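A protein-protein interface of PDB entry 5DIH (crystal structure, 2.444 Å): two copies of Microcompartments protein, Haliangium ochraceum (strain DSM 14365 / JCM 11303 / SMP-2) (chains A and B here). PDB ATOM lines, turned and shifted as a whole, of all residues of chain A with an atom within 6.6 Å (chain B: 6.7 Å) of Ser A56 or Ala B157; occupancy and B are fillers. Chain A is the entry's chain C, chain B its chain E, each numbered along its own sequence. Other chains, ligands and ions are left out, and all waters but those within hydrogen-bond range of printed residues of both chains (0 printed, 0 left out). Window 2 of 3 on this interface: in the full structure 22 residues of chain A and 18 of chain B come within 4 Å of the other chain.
O of Thr A28 is in hydrogen-bond range of NZ of Lys B159 (3.5 Å).
The backbone carbonyl oxygen of Gly A57 lies within hydrogen-bond range of the side-chain amino group of Lys B159 (2.7 Å).
O of Val A54 sits close to O of Gly B155, 3.3 Å away.
OG of Ser B55 is in hydrogen-bond range of N of Gly B155 (2.7 Å).
N of Ala B153 sits at hydrogen-bond distance from O of Lys B159 (2.8 Å).
Among the printed residues, merely in contact across the chains: Ser A55 with Gly B155, Ser A56 with Ala B157, Gly A57 with Ile B156 and Gly A57 with Ala B157.
Of the printed residues of chain B, Thr A28 touches Lys B159.
Printed residues of chain B within 4 Å of Val A54: Gly B155 (3.3 Å).
Ser A56 touches just one residue of chain B: Ala B157.
Printed residues of chain B within 4 Å of Gly A57: Ile B156, Ala B157 and Lys B159.
Ser B56 touches none of the printed residues of chain A.
Ala B157 touches just these residues of chain A: Ser A56 and Gly A57.
Of the printed residues of chain A, Lys B159 touches Thr A28 and Gly A57.
The nearest residue of chain B that does not touch Ser A56 is Gly B155 (4.3 Å).
Printed residues of chain A that touch a printed residue of chain B: Thr A28, Val A54, Ser A55, Ser A56 and Gly A57.
Along chain A the printed residues that touch a printed residue of chain B span positions 28 to 57.
Printed residues of chain B that touch a printed residue of chain A: Gly B155, Ile B156, Ala B157 and Lys B159.
Ser A56 touches Ala B157, but with the chains exchanged Ala A157 does not touch Ser B56 (9.1 Å).
Positions printed for both chains: 55, 56, 58, 153, 156, 157, 158 and 159.
Of the 7 pairs that touch across the chains among the printed residues, none has its exchanged pair printed and touching as well.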
ATOM      1  N   THR A  28      -2.796  28.959  25.099  1.00  0.00           N
ATOM      2  CA  THR A  28      -4.201  29.281  25.328  1.00  0.00           C
ATOM      3  C   THR A  28      -5.056  29.054  24.082  1.00  0.00           C
ATOM      4  O   THR A  28      -6.277  29.205  24.119  1.00  0.00           O
ATOM      5  CB  THR A  28      -4.372  30.742  25.789  1.00  0.00           C
ATOM      6  OG1 THR A  28      -5.718  30.954  26.230  1.00  0.00           O
ATOM      7  CG2 THR A  28      -4.058  31.701  24.650  1.00  0.00           C
ATOM      8  N   VAL A  54      -6.677  20.417  26.658  1.00  0.00           N
ATOM      9  CA  VAL A  54      -7.089  20.128  28.024  1.00  0.00           C
ATOM     10  C   VAL A  54      -8.217  21.055  28.454  1.00  0.00           C
ATOM     11  O   VAL A  54      -8.653  21.911  27.683  1.00  0.00           O
ATOM     12  CB  VAL A  54      -5.910  20.258  29.006  1.00  0.00           C
ATOM     13  CG1 VAL A  54      -4.914  19.129  28.787  1.00  0.00           C
ATOM     14  CG2 VAL A  54      -5.234  21.612  28.849  1.00  0.00           C
ATOM     15  N   SER A  55      -8.688  20.880  29.686  1.00  0.00           N
ATOM     16  CA  SER A  55      -9.794  21.675  30.209  1.00  0.00           C
ATOM     17  C   SER A  55      -9.458  23.162  30.221  1.00  0.00           C
ATOM     18  O   SER A  55      -8.287  23.541  30.160  1.00  0.00           O
ATOM     19  CB  SER A  55     -10.172  21.206  31.614  1.00  0.00           C
ATOM     20  OG  SER A  55     -10.666  19.878  31.589  1.00  0.00           O
ATOM     21  N   SER A  56     -10.502  23.988  30.295  1.00  0.00           N
ATOM     22  CA  SER A  56     -10.409  25.447  30.192  1.00  0.00           C
ATOM     23  C   SER A  56      -9.936  25.881  28.803  1.00  0.00           C
ATOM     24  O   SER A  56      -9.463  27.004  28.618  1.00  0.00           O
ATOM     25  CB  SER A  56      -9.490  26.027  31.275  1.00  0.00           C
ATOM     26  OG  SER A  56      -8.135  25.689  31.038  1.00  0.00           O
ATOM     27  N   GLY A  57     -10.073  24.986  27.829  1.00  0.00           N
ATOM     28  CA  GLY A  57      -9.809  25.311  26.439  1.00  0.00           C
ATOM     29  C   GLY A  57      -8.365  25.645  26.126  1.00  0.00           C
ATOM     30  O   GLY A  57      -8.081  26.376  25.177  1.00  0.00           O
ATOM     31  N   LYS A  58      -7.448  25.107  26.922  1.00  0.00           N
ATOM     32  CA  LYS A  58      -6.028  25.332  26.695  1.00  0.00           C
ATOM     33  C   LYS A  58      -5.416  24.175  25.915  1.00  0.00           C
ATOM     34  O   LYS A  58      -6.005  23.097  25.820  1.00  0.00           O
ATOM     35  CB  LYS A  58      -5.297  25.528  28.024  1.00  0.00           C
ATOM     36  CG  LYS A  58      -5.853  26.667  28.864  1.00  0.00           C
ATOM     37  CD  LYS A  58      -4.988  26.943  30.085  1.00  0.00           C
ATOM     38  CE  LYS A  58      -4.921  25.741  31.011  1.00  0.00           C
ATOM     39  NZ  LYS A  58      -4.149  26.045  32.249  1.00  0.00           N
ATOM     40  N   ALA A 153      -4.364  19.774  34.544  1.00  0.00           N
ATOM     41  CA  ALA A 153      -5.352  20.558  33.797  1.00  0.00           C
ATOM     42  C   ALA A 153      -6.702  19.861  33.614  1.00  0.00           C
ATOM     43  O   ALA A 153      -7.744  20.422  33.955  1.00  0.00           O
ATOM     44  CB  ALA A 153      -4.784  20.957  32.436  1.00  0.00           C
ATOM     45  N   ILE A 156     -10.048  19.750  36.008  1.00  0.00           N
ATOM     46  CA  ILE A 156      -9.955  20.744  37.074  1.00  0.00           C
ATOM     47  C   ILE A 156      -9.658  22.152  36.551  1.00  0.00           C
ATOM     48  O   ILE A 156      -8.884  22.897  37.153  1.00  0.00           O
ATOM     49  CB  ILE A 156      -8.884  20.352  38.108  1.00  0.00           C
ATOM     50  CG1 ILE A 156      -7.592  19.934  37.407  1.00  0.00           C
ATOM     51  CG2 ILE A 156      -9.386  19.214  38.981  1.00  0.00           C
ATOM     52  CD1 ILE A 156      -6.529  19.420  38.350  1.00  0.00           C
ATOM     53  N   ALA A 157     -10.285  22.496  35.427  1.00  0.00           N
ATOM     54  CA  ALA A 157     -10.280  23.856  34.882  1.00  0.00           C
ATOM     55  C   ALA A 157      -8.890  24.398  34.569  1.00  0.00           C
ATOM     56  O   ALA A 157      -8.661  25.605  34.643  1.00  0.00           O
ATOM     57  CB  ALA A 157     -10.998  24.802  35.840  1.00  0.00           C
ATOM     58  N   GLY A 158      -7.965  23.515  34.213  1.00  0.00           N
ATOM     59  CA  GLY A 158      -6.636  23.941  33.814  1.00  0.00           C
ATOM     60  C   GLY A 158      -5.612  23.929  34.933  1.00  0.00           C
ATOM     61  O   GLY A 158      -4.409  23.937  34.677  1.00  0.00           O
ATOM     62  N   LYS A 159      -6.085  23.914  36.175  1.00  0.00           N
ATOM     63  CA  LYS A 159      -5.195  23.848  37.331  1.00  0.00           C
ATOM     64  C   LYS A 159      -4.517  22.483  37.400  1.00  0.00           C
ATOM     65  O   LYS A 159      -4.922  21.551  36.714  1.00  0.00           O
ATOM     66  CB  LYS A 159      -5.969  24.133  38.618  1.00  0.00           C
ATOM     67  CG  LYS A 159      -6.525  25.547  38.699  1.00  0.00           C
ATOM     68  CD  LYS A 159      -7.817  25.623  39.511  1.00  0.00           C
ATOM     69  CE  LYS A 159      -7.593  25.341  40.989  1.00  0.00           C
ATOM     70  NZ  LYS A 159      -7.615  23.888  41.318  1.00  0.00           N
ATOM     71  N   SER B  55     -19.575  21.326  28.608  1.00  0.00           N
ATOM     72  CA  SER B  55     -18.537  22.100  29.342  1.00  0.00           C
ATOM     73  C   SER B  55     -18.691  23.590  29.508  1.00  0.00           C
ATOM     74  O   SER B  55     -18.927  24.308  28.588  1.00  0.00           O
ATOM     75  CB  SER B  55     -17.141  21.791  28.847  1.00  0.00           C
ATOM     76  OG  SER B  55     -16.848  20.437  28.950  1.00  0.00           O
ATOM     77  N   SER B  56     -18.542  24.039  30.729  1.00  0.00           N
ATOM     78  CA  SER B  56     -18.722  25.425  31.100  1.00  0.00           C
ATOM     79  C   SER B  56     -20.200  25.692  31.432  1.00  0.00           C
ATOM     80  O   SER B  56     -20.620  26.799  31.653  1.00  0.00           O
ATOM     81  CB  SER B  56     -18.099  26.393  30.098  1.00  0.00           C
ATOM     82  OG  SER B  56     -18.601  26.199  28.830  1.00  0.00           O
ATOM     83  N   LYS B  58     -22.928  25.018  29.522  1.00  0.00           N
ATOM     84  CA  LYS B  58     -23.835  25.305  28.414  1.00  0.00           C
ATOM     85  C   LYS B  58     -24.684  24.092  28.048  1.00  0.00           C
ATOM     86  O   LYS B  58     -24.294  22.949  28.292  1.00  0.00           O
ATOM     87  CB  LYS B  58     -23.054  25.773  27.184  1.00  0.00           C
ATOM     88  CG  LYS B  58     -22.237  27.031  27.397  1.00  0.00           C
ATOM     89  CD  LYS B  58     -21.683  27.549  26.080  1.00  0.00           C
ATOM     90  CE  LYS B  58     -20.902  26.472  25.345  1.00  0.00           C
ATOM     91  NZ  LYS B  58     -20.314  26.982  24.073  1.00  0.00           N
ATOM     92  N   ALA B 127     -15.462  30.103  18.859  1.00  0.00           N
ATOM     93  CA  ALA B 127     -15.895  30.381  20.223  1.00  0.00           C
ATOM     94  C   ALA B 127     -17.113  29.549  20.626  1.00  0.00           C
ATOM     95  O   ALA B 127     -17.228  29.124  21.777  1.00  0.00           O
ATOM     96  CB  ALA B 127     -16.193  31.863  20.384  1.00  0.00           C
ATOM     97  N   ALA B 153     -17.278  21.870  22.244  1.00  0.00           N
ATOM     98  CA  ALA B 153     -17.489  22.353  23.611  1.00  0.00           C
ATOM     99  C   ALA B 153     -16.946  21.434  24.708  1.00  0.00           C
ATOM    100  O   ALA B 153     -16.207  21.889  25.583  1.00  0.00           O
ATOM    101  CB  ALA B 153     -18.973  22.622  23.845  1.00  0.00           C
ATOM    102  N   ILE B 154     -17.312  20.156  24.664  1.00  0.00           N
ATOM    103  CA  ILE B 154     -16.975  19.218  25.734  1.00  0.00           C
ATOM    104  C   ILE B 154     -15.469  19.116  25.992  1.00  0.00           C
ATOM    105  O   ILE B 154     -14.687  18.767  25.106  1.00  0.00           O
ATOM    106  CB  ILE B 154     -17.544  17.806  25.439  1.00  0.00           C
ATOM    107  CG1 ILE B 154     -16.990  16.783  26.431  1.00  0.00           C
ATOM    108  CG2 ILE B 154     -17.246  17.383  24.011  1.00  0.00           C
ATOM    109  CD1 ILE B 154     -17.457  15.368  26.170  1.00  0.00           C
ATOM    110  N   GLY B 155     -15.072  19.451  27.215  1.00  0.00           N
ATOM    111  CA  GLY B 155     -13.688  19.343  27.633  1.00  0.00           C
ATOM    112  C   GLY B 155     -12.830  20.553  27.317  1.00  0.00           C
ATOM    113  O   GLY B 155     -11.706  20.660  27.803  1.00  0.00           O
ATOM    114  N   ILE B 156     -13.348  21.468  26.503  1.00  0.00           N
ATOM    115  CA  ILE B 156     -12.566  22.631  26.097  1.00  0.00           C
ATOM    116  C   ILE B 156     -13.293  23.950  26.349  1.00  0.00           C
ATOM    117  O   ILE B 156     -13.259  24.859  25.517  1.00  0.00           O
ATOM    118  CB  ILE B 156     -12.170  22.546  24.612  1.00  0.00           C
ATOM    119  CG1 ILE B 156     -13.392  22.256  23.740  1.00  0.00           C
ATOM    120  CG2 ILE B 156     -11.122  21.465  24.408  1.00  0.00           C
ATOM    121  CD1 ILE B 156     -13.077  22.213  22.259  1.00  0.00           C
ATOM    122  N   ALA B 157     -13.946  24.037  27.505  1.00  0.00           N
ATOM    123  CA  ALA B 157     -14.548  25.278  27.993  1.00  0.00           C
ATOM    124  C   ALA B 157     -15.553  25.897  27.027  1.00  0.00           C
ATOM    125  O   ALA B 157     -15.675  27.120  26.952  1.00  0.00           O
ATOM    126  CB  ALA B 157     -13.457  26.290  28.323  1.00  0.00           C
ATOM    127  N   GLY B 158     -16.274  25.058  26.292  1.00  0.00           N
ATOM    128  CA  GLY B 158     -17.325  25.542  25.415  1.00  0.00           C
ATOM    129  C   GLY B 158     -16.859  25.928  24.024  1.00  0.00           C
ATOM    130  O   GLY B 158     -17.678  26.116  23.123  1.00  0.00           O
ATOM    131  N   LYS B 159     -15.549  26.048  23.840  1.00  0.00           N
ATOM    132  CA  LYS B 159     -14.997  26.385  22.530  1.00  0.00           C
ATOM    133  C   LYS B 159     -15.169  25.217  21.564  1.00  0.00           C
ATOM    134  O   LYS B 159     -15.685  24.167  21.937  1.00  0.00           O
ATOM    135  CB  LYS B 159     -13.519  26.769  22.644  1.00  0.00           C
ATOM    136  CG  LYS B 159     -13.247  27.898  23.623  1.00  0.00           C
ATOM    137  CD  LYS B 159     -11.850  28.466  23.444  1.00  0.00           C
ATOM    138  CE  LYS B 159     -10.787  27.387  23.551  1.00  0.00           C
ATOM    139  NZ  LYS B 159      -9.417  27.938  23.351  1.00  0.00           N
